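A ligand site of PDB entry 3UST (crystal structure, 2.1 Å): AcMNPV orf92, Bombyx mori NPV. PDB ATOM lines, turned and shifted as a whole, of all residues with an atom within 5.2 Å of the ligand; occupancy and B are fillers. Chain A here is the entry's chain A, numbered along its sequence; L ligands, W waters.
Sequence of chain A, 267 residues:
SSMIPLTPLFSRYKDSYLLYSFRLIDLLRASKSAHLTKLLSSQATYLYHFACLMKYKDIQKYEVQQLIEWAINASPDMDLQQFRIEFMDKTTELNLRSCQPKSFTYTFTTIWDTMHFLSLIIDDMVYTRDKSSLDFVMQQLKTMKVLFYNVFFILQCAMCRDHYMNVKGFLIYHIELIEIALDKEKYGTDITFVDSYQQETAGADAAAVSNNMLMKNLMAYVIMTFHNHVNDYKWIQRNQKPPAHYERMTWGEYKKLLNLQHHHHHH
OD1 of Asn 228 lies within hydrogen-bond range of N3 of the ligand (2.9 Å).
O of Met 224 is in hydrogen-bond range of N3 of the ligand (2.8 Å).
The indole nitrogen (NE1) of Trp 112 is in hydrogen-bond range of an oxygen (O9) of the ligand, at 2.9 Å.
O11 of the ligand lies within hydrogen-bond range of NZ of Lys 234 (2.6 Å).
An oxygen (O2) of the ligand lies within hydrogen-bond range of a ring nitrogen (NE2) of His 227 (2.6 Å).
The side-chain hydroxyl (OG1) of Thr 109 lies close to an oxygen (O1) of the ligand (3.4 Å).
A nitrogen (N7) of the ligand lies within hydrogen-bond range of the side-chain amide oxygen (OE1) of Gln 237, 2.9 Å away.
ND2 of Asn 231 is in hydrogen-bond range of O9 of the ligand (2.7 Å).
ND1 of His 163 sits at hydrogen-bond distance from O8 of the ligand, 2.9 Å away.
Water W7 bridges O5 of the ligand (2.7 Å) and NH1 of Arg 12 (3.3 Å).
Water W10 bridges OH of Tyr 13 (2.5 Å) and N5 of the ligand (2.8 Å).
Water W5 lies within hydrogen-bond range of the side-chain hydroxyl (OG1) of Thr 109 (2.5 Å) and an oxygen (O14) of the ligand (3.1 Å).
ND1 of His 116 lies within hydrogen-bond range of OH of Tyr 254 (3.0 Å).
O of Met 249 lies within hydrogen-bond range of ND2 of Asn 228 (2.9 Å).
SG of Cys 160 forms a disulfide with SG of Cys 157.
OH of Tyr 13 lies within hydrogen-bond range of OH of Tyr 254.
ND1 of His 227 is in hydrogen-bond range of NE2 of His 116 (2.9 Å).
SG of Cys 160 sits close to N9 of the ligand.
NH1 of Arg 12 touches O5 of the ligand (3.8 Å).
Phe 108 touches the ligand (CB to O10, 3.4 Å).
Ile 111 touches the ligand (CG2 to C19, 3.8 Å).
Met 115 touches the ligand.
NE2 of His 116 touches C9 of the ligand, 3.3 Å away.
CE1 of Phe 153 touches C16 of the ligand, 3.4 Å away.
O of Met 159 touches O8 of the ligand (3.7 Å).
Tyr 164 touches the ligand.
Val 230 touches the ligand.
Met 249 touches the ligand.
CE1 of Tyr 254 touches C9 of the ligand, at 3.4 Å.
Hydrophobic or aromatic side chains that line the ligand: Phe 108, Ile 111, Trp 112, Met 115, His 116, Phe 153, Met 159, His 163, Tyr 164, Met 224, His 227, Val 230, Met 249 and Tyr 254.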
ATOM      1  N   ARG A  12     -19.122  13.449 -10.629  1.00  0.00           N
ATOM      2  CA  ARG A  12     -18.901  14.697 -11.343  1.00  0.00           C
ATOM      3  C   ARG A  12     -17.415  15.059 -11.306  1.00  0.00           C
ATOM      4  O   ARG A  12     -16.850  15.482 -12.329  1.00  0.00           O
ATOM      5  CB  ARG A  12     -19.773  15.831 -10.782  1.00  0.00           C
ATOM      6  CG  ARG A  12     -19.871  17.024 -11.750  1.00  0.00           C
ATOM      7  CD  ARG A  12     -20.464  18.256 -11.074  1.00  0.00           C
ATOM      8  NE  ARG A  12     -19.487  19.024 -10.300  1.00  0.00           N
ATOM      9  CZ  ARG A  12     -19.792  19.765  -9.245  1.00  0.00           C
ATOM     10  NH1 ARG A  12     -21.041  19.813  -8.773  1.00  0.00           N
ATOM     11  NH2 ARG A  12     -18.859  20.457  -8.633  1.00  0.00           N
ATOM     12  N   TYR A  13     -16.779  14.876 -10.138  1.00  0.00           N
ATOM     13  CA  TYR A  13     -15.329  15.150  -9.976  1.00  0.00           C
ATOM     14  C   TYR A  13     -14.490  14.354 -10.972  1.00  0.00           C
ATOM     15  O   TYR A  13     -13.620  14.907 -11.691  1.00  0.00           O
ATOM     16  CB  TYR A  13     -14.884  14.850  -8.524  1.00  0.00           C
ATOM     17  CG  TYR A  13     -15.330  15.877  -7.471  1.00  0.00           C
ATOM     18  CD1 TYR A  13     -15.966  17.070  -7.824  1.00  0.00           C
ATOM     19  CD2 TYR A  13     -15.045  15.666  -6.126  1.00  0.00           C
ATOM     20  CE1 TYR A  13     -16.352  18.023  -6.851  1.00  0.00           C
ATOM     21  CE2 TYR A  13     -15.397  16.604  -5.159  1.00  0.00           C
ATOM     22  CZ  TYR A  13     -16.040  17.789  -5.531  1.00  0.00           C
ATOM     23  OH  TYR A  13     -16.410  18.715  -4.568  1.00  0.00           O
ATOM     24  N   PHE A 108     -14.281  27.019 -14.923  1.00  0.00           N
ATOM     25  CA  PHE A 108     -13.528  27.027 -13.660  1.00  0.00           C
ATOM     26  C   PHE A 108     -13.890  25.842 -12.751  1.00  0.00           C
ATOM     27  O   PHE A 108     -13.042  25.322 -12.030  1.00  0.00           O
ATOM     28  CB  PHE A 108     -13.763  28.312 -12.876  1.00  0.00           C
ATOM     29  CG  PHE A 108     -13.103  29.529 -13.451  1.00  0.00           C
ATOM     30  CD1 PHE A 108     -11.727  29.682 -13.374  1.00  0.00           C
ATOM     31  CD2 PHE A 108     -13.852  30.515 -14.062  1.00  0.00           C
ATOM     32  CE1 PHE A 108     -11.099  30.804 -13.874  1.00  0.00           C
ATOM     33  CE2 PHE A 108     -13.260  31.644 -14.584  1.00  0.00           C
ATOM     34  CZ  PHE A 108     -11.866  31.800 -14.494  1.00  0.00           C
ATOM     35  N   THR A 109     -15.161  25.465 -12.759  1.00  0.00           N
ATOM     36  CA  THR A 109     -15.630  24.358 -11.950  1.00  0.00           C
ATOM     37  C   THR A 109     -14.942  23.045 -12.314  1.00  0.00           C
ATOM     38  O   THR A 109     -14.705  22.204 -11.450  1.00  0.00           O
ATOM     39  CB  THR A 109     -17.155  24.236 -12.020  1.00  0.00           C
ATOM     40  OG1 THR A 109     -17.717  25.383 -11.383  1.00  0.00           O
ATOM     41  CG2 THR A 109     -17.693  23.000 -11.293  1.00  0.00           C
ATOM     42  N   ILE A 111     -11.839  22.760 -13.252  1.00  0.00           N
ATOM     43  CA  ILE A 111     -10.520  22.822 -12.619  1.00  0.00           C
ATOM     44  C   ILE A 111     -10.610  22.574 -11.116  1.00  0.00           C
ATOM     45  O   ILE A 111      -9.796  21.847 -10.562  1.00  0.00           O
ATOM     46  CB  ILE A 111      -9.795  24.192 -12.848  1.00  0.00           C
ATOM     47  CG1 ILE A 111      -9.823  24.588 -14.315  1.00  0.00           C
ATOM     48  CG2 ILE A 111      -8.327  24.128 -12.324  1.00  0.00           C
ATOM     49  CD1 ILE A 111      -9.473  26.098 -14.559  1.00  0.00           C
ATOM     50  N   TRP A 112     -11.588  23.202 -10.459  1.00  0.00           N
ATOM     51  CA  TRP A 112     -11.860  22.972  -9.023  1.00  0.00           C
ATOM     52  C   TRP A 112     -12.190  21.498  -8.731  1.00  0.00           C
ATOM     53  O   TRP A 112     -11.618  20.917  -7.829  1.00  0.00           O
ATOM     54  CB  TRP A 112     -13.015  23.876  -8.532  1.00  0.00           C
ATOM     55  CG  TRP A 112     -12.604  25.298  -8.191  1.00  0.00           C
ATOM     56  CD1 TRP A 112     -13.188  26.457  -8.654  1.00  0.00           C
ATOM     57  CD2 TRP A 112     -11.573  25.697  -7.274  1.00  0.00           C
ATOM     58  NE1 TRP A 112     -12.546  27.551  -8.101  1.00  0.00           N
ATOM     59  CE2 TRP A 112     -11.565  27.115  -7.254  1.00  0.00           C
ATOM     60  CE3 TRP A 112     -10.661  24.993  -6.462  1.00  0.00           C
ATOM     61  CZ2 TRP A 112     -10.668  27.842  -6.459  1.00  0.00           C
ATOM     62  CZ3 TRP A 112      -9.764  25.720  -5.667  1.00  0.00           C
ATOM     63  CH2 TRP A 112      -9.774  27.132  -5.673  1.00  0.00           C
ATOM     64  N   MET A 115      -9.084  19.406  -8.813  1.00  0.00           N
ATOM     65  CA  MET A 115      -8.386  19.565  -7.532  1.00  0.00           C
ATOM     66  C   MET A 115      -9.067  18.828  -6.414  1.00  0.00           C
ATOM     67  O   MET A 115      -8.404  18.187  -5.641  1.00  0.00           O
ATOM     68  CB  MET A 115      -8.258  21.033  -7.194  1.00  0.00           C
ATOM     69  CG  MET A 115      -7.430  21.728  -8.236  1.00  0.00           C
ATOM     70  SD  MET A 115      -7.124  23.615  -7.934  1.00  0.00           S
ATOM     71  CE  MET A 115      -6.320  23.550  -6.286  1.00  0.00           C
ATOM     72  N   HIS A 116     -10.392  18.903  -6.344  1.00  0.00           N
ATOM     73  CA  HIS A 116     -11.100  18.132  -5.305  1.00  0.00           C
ATOM     74  C   HIS A 116     -10.956  16.626  -5.494  1.00  0.00           C
ATOM     75  O   HIS A 116     -10.828  15.880  -4.517  1.00  0.00           O
ATOM     76  CB  HIS A 116     -12.551  18.539  -5.176  1.00  0.00           C
ATOM     77  CG  HIS A 116     -12.742  19.952  -4.722  1.00  0.00           C
ATOM     78  ND1 HIS A 116     -12.308  20.398  -3.489  1.00  0.00           N
ATOM     79  CD2 HIS A 116     -13.293  21.029  -5.335  1.00  0.00           C
ATOM     80  CE1 HIS A 116     -12.579  21.688  -3.359  1.00  0.00           C
ATOM     81  NE2 HIS A 116     -13.180  22.095  -4.465  1.00  0.00           N
ATOM     82  N   PHE A 153      -4.237  26.560 -16.216  1.00  0.00           N
ATOM     83  CA  PHE A 153      -5.624  26.989 -16.212  1.00  0.00           C
ATOM     84  C   PHE A 153      -6.388  26.609 -17.488  1.00  0.00           C
ATOM     85  O   PHE A 153      -7.564  26.240 -17.430  1.00  0.00           O
ATOM     86  CB  PHE A 153      -5.755  28.477 -15.845  1.00  0.00           C
ATOM     87  CG  PHE A 153      -5.700  28.727 -14.364  1.00  0.00           C
ATOM     88  CD1 PHE A 153      -6.872  28.799 -13.610  1.00  0.00           C
ATOM     89  CD2 PHE A 153      -4.472  28.778 -13.710  1.00  0.00           C
ATOM     90  CE1 PHE A 153      -6.811  28.983 -12.231  1.00  0.00           C
ATOM     91  CE2 PHE A 153      -4.411  28.951 -12.321  1.00  0.00           C
ATOM     92  CZ  PHE A 153      -5.583  29.058 -11.582  1.00  0.00           C
ATOM     93  N   CYS A 157      -7.252  33.499 -17.583  1.00  0.00           N
ATOM     94  CA  CYS A 157      -7.446  34.322 -16.394  1.00  0.00           C
ATOM     95  C   CYS A 157      -6.085  34.627 -15.813  1.00  0.00           C
ATOM     96  O   CYS A 157      -5.519  33.823 -15.077  1.00  0.00           O
ATOM     97  CB  CYS A 157      -8.328  33.584 -15.375  1.00  0.00           C
ATOM     98  SG  CYS A 157      -8.662  34.552 -13.892  1.00  0.00           S
ATOM     99  N   MET A 159      -5.224  36.999 -13.776  1.00  0.00           N
ATOM    100  CA  MET A 159      -5.449  37.212 -12.346  1.00  0.00           C
ATOM    101  C   MET A 159      -5.419  35.897 -11.557  1.00  0.00           C
ATOM    102  O   MET A 159      -4.821  35.856 -10.485  1.00  0.00           O
ATOM    103  CB  MET A 159      -6.790  37.897 -12.165  1.00  0.00           C
ATOM    104  CG  MET A 159      -7.296  37.917 -10.755  1.00  0.00           C
ATOM    105  SD  MET A 159      -8.929  38.990 -10.637  1.00  0.00           S
ATOM    106  CE  MET A 159      -8.003  40.726 -10.628  1.00  0.00           C
ATOM    107  N   CYS A 160      -6.088  34.863 -12.086  1.00  0.00           N
ATOM    108  CA  CYS A 160      -6.100  33.534 -11.466  1.00  0.00           C
ATOM    109  C   CYS A 160      -4.693  32.941 -11.366  1.00  0.00           C
ATOM    110  O   CYS A 160      -4.299  32.427 -10.304  1.00  0.00           O
ATOM    111  CB  CYS A 160      -7.034  32.562 -12.230  1.00  0.00           C
ATOM    112  SG  CYS A 160      -8.746  33.151 -12.437  1.00  0.00           S
ATOM    113  N   HIS A 163      -2.477  34.720  -8.856  1.00  0.00           N
ATOM    114  CA  HIS A 163      -2.961  34.484  -7.503  1.00  0.00           C
ATOM    115  C   HIS A 163      -2.572  33.073  -7.044  1.00  0.00           C
ATOM    116  O   HIS A 163      -2.082  32.890  -5.912  1.00  0.00           O
ATOM    117  CB  HIS A 163      -4.463  34.698  -7.414  1.00  0.00           C
ATOM    118  CG  HIS A 163      -5.018  34.568  -6.017  1.00  0.00           C
ATOM    119  ND1 HIS A 163      -6.329  34.214  -5.774  1.00  0.00           N
ATOM    120  CD2 HIS A 163      -4.434  34.706  -4.806  1.00  0.00           C
ATOM    121  CE1 HIS A 163      -6.524  34.162  -4.471  1.00  0.00           C
ATOM    122  NE2 HIS A 163      -5.394  34.445  -3.867  1.00  0.00           N
ATOM    123  N   TYR A 164      -2.776  32.091  -7.914  1.00  0.00           N
ATOM    124  CA  TYR A 164      -2.394  30.716  -7.623  1.00  0.00           C
ATOM    125  C   TYR A 164      -0.885  30.596  -7.458  1.00  0.00           C
ATOM    126  O   TYR A 164      -0.426  29.868  -6.574  1.00  0.00           O
ATOM    127  CB  TYR A 164      -2.920  29.761  -8.702  1.00  0.00           C
ATOM    128  CG  TYR A 164      -2.737  28.312  -8.317  1.00  0.00           C
ATOM    129  CD1 TYR A 164      -3.561  27.705  -7.347  1.00  0.00           C
ATOM    130  CD2 TYR A 164      -1.746  27.542  -8.919  1.00  0.00           C
ATOM    131  CE1 TYR A 164      -3.389  26.367  -6.988  1.00  0.00           C
ATOM    132  CE2 TYR A 164      -1.575  26.215  -8.570  1.00  0.00           C
ATOM    133  CZ  TYR A 164      -2.364  25.644  -7.603  1.00  0.00           C
ATOM    134  OH  TYR A 164      -2.155  24.329  -7.324  1.00  0.00           O
ATOM    135  N   ILE A 223      -8.540  21.485   0.526  1.00  0.00           N
ATOM    136  CA  ILE A 223      -8.881  22.079  -0.762  1.00  0.00           C
ATOM    137  C   ILE A 223     -10.275  22.720  -0.728  1.00  0.00           C
ATOM    138  O   ILE A 223     -10.502  23.701  -1.421  1.00  0.00           O
ATOM    139  CB  ILE A 223      -8.603  21.101  -1.963  1.00  0.00           C
ATOM    140  CG1 ILE A 223      -7.125  20.599  -1.852  1.00  0.00           C
ATOM    141  CG2 ILE A 223      -8.889  21.783  -3.325  1.00  0.00           C
ATOM    142  CD1 ILE A 223      -6.558  19.905  -3.113  1.00  0.00           C
ATOM    143  N   MET A 224     -11.194  22.160   0.069  1.00  0.00           N
ATOM    144  CA  MET A 224     -12.469  22.823   0.288  1.00  0.00           C
ATOM    145  C   MET A 224     -12.210  24.209   0.864  1.00  0.00           C
ATOM    146  O   MET A 224     -12.835  25.159   0.438  1.00  0.00           O
ATOM    147  CB  MET A 224     -13.353  22.051   1.271  1.00  0.00           C
ATOM    148  CG  MET A 224     -14.747  22.716   1.423  1.00  0.00           C
ATOM    149  SD  MET A 224     -15.649  22.438   3.127  1.00  0.00           S
ATOM    150  CE  MET A 224     -14.621  23.587   4.252  1.00  0.00           C
ATOM    151  N   THR A 225     -11.346  24.272   1.883  1.00  0.00           N
ATOM    152  CA  THR A 225     -10.947  25.522   2.528  1.00  0.00           C
ATOM    153  C   THR A 225     -10.268  26.511   1.554  1.00  0.00           C
ATOM    154  O   THR A 225     -10.552  27.715   1.553  1.00  0.00           O
ATOM    155  CB  THR A 225      -9.984  25.213   3.695  1.00  0.00           C
ATOM    156  OG1 THR A 225     -10.705  24.471   4.685  1.00  0.00           O
ATOM    157  CG2 THR A 225      -9.447  26.479   4.300  1.00  0.00           C
ATOM    158  N   PHE A 226      -9.351  25.988   0.774  1.00  0.00           N
ATOM    159  CA  PHE A 226      -8.664  26.781  -0.211  1.00  0.00           C
ATOM    160  C   PHE A 226      -9.658  27.318  -1.249  1.00  0.00           C
ATOM    161  O   PHE A 226      -9.542  28.449  -1.683  1.00  0.00           O
ATOM    162  CB  PHE A 226      -7.603  25.901  -0.871  1.00  0.00           C
ATOM    163  CG  PHE A 226      -6.726  26.616  -1.862  1.00  0.00           C
ATOM    164  CD1 PHE A 226      -5.678  27.400  -1.445  1.00  0.00           C
ATOM    165  CD2 PHE A 226      -6.953  26.464  -3.233  1.00  0.00           C
ATOM    166  CE1 PHE A 226      -4.846  28.033  -2.378  1.00  0.00           C
ATOM    167  CE2 PHE A 226      -6.166  27.069  -4.143  1.00  0.00           C
ATOM    168  CZ  PHE A 226      -5.090  27.861  -3.729  1.00  0.00           C
ATOM    169  N   HIS A 227     -10.652  26.506  -1.626  1.00  0.00           N
ATOM    170  CA  HIS A 227     -11.632  26.894  -2.658  1.00  0.00           C
ATOM    171  C   HIS A 227     -12.503  28.051  -2.103  1.00  0.00           C
ATOM    172  O   HIS A 227     -12.765  29.020  -2.799  1.00  0.00           O
ATOM    173  CB  HIS A 227     -12.455  25.633  -3.083  1.00  0.00           C
ATOM    174  CG  HIS A 227     -13.451  25.854  -4.199  1.00  0.00           C
ATOM    175  ND1 HIS A 227     -13.985  24.792  -4.918  1.00  0.00           N
ATOM    176  CD2 HIS A 227     -14.042  26.967  -4.680  1.00  0.00           C
ATOM    177  CE1 HIS A 227     -14.863  25.257  -5.799  1.00  0.00           C
ATOM    178  NE2 HIS A 227     -14.904  26.570  -5.693  1.00  0.00           N
ATOM    179  N   ASN A 228     -12.937  27.968  -0.847  1.00  0.00           N
ATOM    180  CA  ASN A 228     -13.614  29.108  -0.203  1.00  0.00           C
ATOM    181  C   ASN A 228     -12.784  30.377  -0.130  1.00  0.00           C
ATOM    182  O   ASN A 228     -13.287  31.471  -0.334  1.00  0.00           O
ATOM    183  CB  ASN A 228     -14.050  28.746   1.221  1.00  0.00           C
ATOM    184  CG  ASN A 228     -15.258  27.848   1.246  1.00  0.00           C
ATOM    185  OD1 ASN A 228     -16.119  27.901   0.360  1.00  0.00           O
ATOM    186  ND2 ASN A 228     -15.375  27.058   2.319  1.00  0.00           N
ATOM    187  N   VAL A 230     -10.174  31.318  -2.082  1.00  0.00           N
ATOM    188  CA  VAL A 230     -10.065  31.940  -3.406  1.00  0.00           C
ATOM    189  C   VAL A 230     -11.329  32.721  -3.826  1.00  0.00           C
ATOM    190  O   VAL A 230     -11.239  33.854  -4.339  1.00  0.00           O
ATOM    191  CB  VAL A 230      -9.631  30.909  -4.442  1.00  0.00           C
ATOM    192  CG1 VAL A 230      -9.775  31.448  -5.836  1.00  0.00           C
ATOM    193  CG2 VAL A 230      -8.148  30.488  -4.133  1.00  0.00           C
ATOM    194  N   ASN A 231     -12.492  32.141  -3.558  1.00  0.00           N
ATOM    195  CA  ASN A 231     -13.766  32.812  -3.806  1.00  0.00           C
ATOM    196  C   ASN A 231     -14.024  34.020  -2.886  1.00  0.00           C
ATOM    197  O   ASN A 231     -14.661  34.972  -3.320  1.00  0.00           O
ATOM    198  CB  ASN A 231     -14.925  31.816  -3.702  1.00  0.00           C
ATOM    199  CG  ASN A 231     -15.081  30.954  -4.953  1.00  0.00           C
ATOM    200  OD1 ASN A 231     -15.848  29.974  -4.989  1.00  0.00           O
ATOM    201  ND2 ASN A 231     -14.367  31.319  -5.991  1.00  0.00           N
ATOM    202  N   LYS A 234     -11.618  36.734  -4.281  1.00  0.00           N
ATOM    203  CA  LYS A 234     -11.918  37.346  -5.560  1.00  0.00           C
ATOM    204  C   LYS A 234     -12.744  38.638  -5.431  1.00  0.00           C
ATOM    205  O   LYS A 234     -12.578  39.554  -6.238  1.00  0.00           O
ATOM    206  CB  LYS A 234     -12.487  36.350  -6.569  1.00  0.00           C
ATOM    207  CG  LYS A 234     -13.947  36.150  -6.456  1.00  0.00           C
ATOM    208  CD  LYS A 234     -14.473  35.253  -7.557  1.00  0.00           C
ATOM    209  CE  LYS A 234     -15.703  34.510  -7.058  1.00  0.00           C
ATOM    210  NZ  LYS A 234     -16.428  33.925  -8.193  1.00  0.00           N
ATOM    211  N   GLN A 237     -10.181  41.309  -4.801  1.00  0.00           N
ATOM    212  CA  GLN A 237      -9.525  41.622  -6.079  1.00  0.00           C
ATOM    213  C   GLN A 237     -10.354  42.581  -6.912  1.00  0.00           C
ATOM    214  O   GLN A 237      -9.819  43.535  -7.484  1.00  0.00           O
ATOM    215  CB  GLN A 237      -9.250  40.362  -6.879  1.00  0.00           C
ATOM    216  CG  GLN A 237      -8.091  39.545  -6.329  1.00  0.00           C
ATOM    217  CD  GLN A 237      -8.107  38.142  -6.869  1.00  0.00           C
ATOM    218  OE1 GLN A 237      -9.170  37.552  -7.069  1.00  0.00           O
ATOM    219  NE2 GLN A 237      -6.942  37.590  -7.131  1.00  0.00           N
ATOM    220  N   ARG A 238     -11.661  42.308  -6.964  1.00  0.00           N
ATOM    221  CA  ARG A 238     -12.633  43.095  -7.706  1.00  0.00           C
ATOM    222  C   ARG A 238     -12.991  44.383  -6.967  1.00  0.00           C
ATOM    223  O   ARG A 238     -13.687  45.222  -7.509  1.00  0.00           O
ATOM    224  CB  ARG A 238     -13.915  42.269  -7.934  1.00  0.00           C
ATOM    225  CG  ARG A 238     -13.746  41.161  -8.961  1.00  0.00           C
ATOM    226  CD  ARG A 238     -15.003  40.292  -9.122  1.00  0.00           C
ATOM    227  NE  ARG A 238     -14.693  39.113  -9.950  1.00  0.00           N
ATOM    228  CZ  ARG A 238     -15.596  38.265 -10.461  1.00  0.00           C
ATOM    229  NH1 ARG A 238     -16.901  38.410 -10.234  1.00  0.00           N
ATOM    230  NH2 ARG A 238     -15.177  37.264 -11.227  1.00  0.00           N
ATOM    231  N   MET A 249     -18.994  26.997   1.080  1.00  0.00           N
ATOM    232  CA  MET A 249     -19.254  25.597   1.366  1.00  0.00           C
ATOM    233  C   MET A 249     -18.865  25.384   2.830  1.00  0.00           C
ATOM    234  O   MET A 249     -17.832  25.875   3.267  1.00  0.00           O
ATOM    235  CB  MET A 249     -18.378  24.732   0.451  1.00  0.00           C
ATOM    236  CG  MET A 249     -18.486  23.242   0.677  1.00  0.00           C
ATOM    237  SD  MET A 249     -20.284  22.517   0.378  1.00  0.00           S
ATOM    238  CE  MET A 249     -20.235  22.444  -1.527  1.00  0.00           C
ATOM    239  N   TYR A 254     -20.204  19.429   3.141  1.00  0.00           N
ATOM    240  CA  TYR A 254     -19.250  18.837   2.194  1.00  0.00           C
ATOM    241  C   TYR A 254     -19.027  17.366   2.450  1.00  0.00           C
ATOM    242  O   TYR A 254     -19.058  16.573   1.527  1.00  0.00           O
ATOM    243  CB  TYR A 254     -17.921  19.572   2.230  1.00  0.00           C
ATOM    244  CG  TYR A 254     -17.080  19.396   0.964  1.00  0.00           C
ATOM    245  CD1 TYR A 254     -17.609  19.675  -0.290  1.00  0.00           C
ATOM    246  CD2 TYR A 254     -15.759  18.961   1.038  1.00  0.00           C
ATOM    247  CE1 TYR A 254     -16.839  19.504  -1.467  1.00  0.00           C
ATOM    248  CE2 TYR A 254     -14.972  18.803  -0.135  1.00  0.00           C
ATOM    249  CZ  TYR A 254     -15.523  19.070  -1.371  1.00  0.00           C
ATOM    250  OH  TYR A 254     -14.740  18.927  -2.518  1.00  0.00           O
HETATM  251  P1  LIG L   1     -17.329  28.047  -8.184  1.00  0.00           P
HETATM  252  O1  LIG L   1     -16.429  27.886  -9.405  1.00  0.00           O
HETATM  253  O2  LIG L   1     -16.520  28.101  -6.957  1.00  0.00           O
HETATM  254  O3  LIG L   1     -18.394  26.865  -7.982  1.00  0.00           O
HETATM  255  C1  LIG L   1     -18.413  25.643  -8.660  1.00  0.00           C
HETATM  256  C2  LIG L   1     -18.989  24.520  -7.791  1.00  0.00           C
HETATM  257  O4  LIG L   1     -18.232  24.387  -6.626  1.00  0.00           O
HETATM  258  C3  LIG L   1     -20.433  24.677  -7.320  1.00  0.00           C
HETATM  259  O5  LIG L   1     -21.029  23.393  -7.438  1.00  0.00           O
HETATM  260  C4  LIG L   1     -20.338  24.956  -5.841  1.00  0.00           C
HETATM  261  O6  LIG L   1     -21.391  24.298  -5.175  1.00  0.00           O
HETATM  262  C5  LIG L   1     -19.034  24.286  -5.449  1.00  0.00           C
HETATM  263  N1  LIG L   1     -18.269  24.894  -4.343  1.00  0.00           N
HETATM  264  C6  LIG L   1     -18.294  26.186  -3.898  1.00  0.00           C
HETATM  265  N2  LIG L   1     -17.384  26.331  -2.887  1.00  0.00           N
HETATM  266  C7  LIG L   1     -16.784  25.131  -2.684  1.00  0.00           C
HETATM  267  C8  LIG L   1     -15.800  24.705  -1.795  1.00  0.00           C
HETATM  268  N3  LIG L   1     -15.167  25.559  -0.981  1.00  0.00           N
HETATM  269  N4  LIG L   1     -15.370  23.395  -1.849  1.00  0.00           N
HETATM  270  C9  LIG L   1     -15.921  22.521  -2.749  1.00  0.00           C
HETATM  271  N5  LIG L   1     -16.886  22.950  -3.625  1.00  0.00           N
HETATM  272  C10 LIG L   1     -17.319  24.240  -3.603  1.00  0.00           C
HETATM  273  N6  LIG L   1     -11.179  33.805  -9.757  1.00  0.00           N
HETATM  274  C11 LIG L   1     -10.842  35.123  -9.482  1.00  0.00           C
HETATM  275  O7  LIG L   1     -11.637  36.006  -9.695  1.00  0.00           O
HETATM  276  N7  LIG L   1      -9.601  35.451  -8.988  1.00  0.00           N
HETATM  277  C12 LIG L   1      -8.664  34.494  -8.714  1.00  0.00           C
HETATM  278  O8  LIG L   1      -7.575  34.891  -8.265  1.00  0.00           O
HETATM  279  C13 LIG L   1      -8.985  33.161  -8.994  1.00  0.00           C
HETATM  280  N8  LIG L   1      -8.070  32.127  -8.780  1.00  0.00           N
HETATM  281  C14 LIG L   1      -8.413  30.817  -9.057  1.00  0.00           C
HETATM  282  C15 LIG L   1      -7.496  29.806  -8.798  1.00  0.00           C
HETATM  283  C16 LIG L   1      -7.826  28.472  -9.048  1.00  0.00           C
HETATM  284  C17 LIG L   1      -6.794  27.382  -8.783  1.00  0.00           C
HETATM  285  C18 LIG L   1      -9.097  28.154  -9.572  1.00  0.00           C
HETATM  286  C19 LIG L   1      -9.473  26.748  -9.897  1.00  0.00           C
HETATM  287  C20 LIG L   1     -10.026  29.171  -9.824  1.00  0.00           C
HETATM  288  C21 LIG L   1      -9.683  30.505  -9.553  1.00  0.00           C
HETATM  289  N9  LIG L   1     -10.593  31.528  -9.779  1.00  0.00           N
HETATM  290  C22 LIG L   1     -10.256  32.833  -9.508  1.00  0.00           C
HETATM  291  C23 LIG L   1     -12.030  31.201 -10.132  1.00  0.00           C
HETATM  292  C24 LIG L   1     -13.021  31.273  -8.972  1.00  0.00           C
HETATM  293  O9  LIG L   1     -12.559  30.490  -7.878  1.00  0.00           O
HETATM  294  C25 LIG L   1     -14.411  30.779  -9.390  1.00  0.00           C
HETATM  295  O10 LIG L   1     -14.342  29.426  -9.735  1.00  0.00           O
HETATM  296  C26 LIG L   1     -15.022  31.525 -10.569  1.00  0.00           C
HETATM  297  O11 LIG L   1     -15.097  32.890 -10.211  1.00  0.00           O
HETATM  298  C27 LIG L   1     -16.438  31.030 -10.905  1.00  0.00           C
HETATM  299  O12 LIG L   1     -17.238  31.163  -9.748  1.00  0.00           O
HETATM  300  P2  LIG L   1     -18.579  30.315  -9.502  1.00  0.00           P
HETATM  301  O13 LIG L   1     -19.633  31.252  -8.958  1.00  0.00           O
HETATM  302  O14 LIG L   1     -19.041  29.687 -10.793  1.00  0.00           O
HETATM  303  O15 LIG L   1     -18.269  29.325  -8.272  1.00  0.00           O
HETATM  304  O   HOH W   1     -19.691  29.261  -4.767  1.00  0.00           O
HETATM  305  O   HOH W   2     -16.994  29.266  -2.444  1.00  0.00           O
HETATM  306  O   HOH W   3     -21.654  23.421 -10.090  1.00  0.00           O
HETATM  307  O   HOH W   4     -20.972  28.003 -11.179  1.00  0.00           O
HETATM  308  O   HOH W   5     -17.576  27.579 -12.615  1.00  0.00           O
HETATM  309  O   HOH W   6      -9.257  34.834  -5.775  1.00  0.00           O
HETATM  310  O   HOH W   7     -20.620  21.251  -5.846  1.00  0.00           O
HETATM  311  O   HOH W   8     -15.937  22.228  -7.495  1.00  0.00           O
HETATM  312  O   HOH W   9     -12.794  34.256 -12.548  1.00  0.00           O
HETATM  313  O   HOH W  10     -17.670  20.772  -5.283  1.00  0.00           O
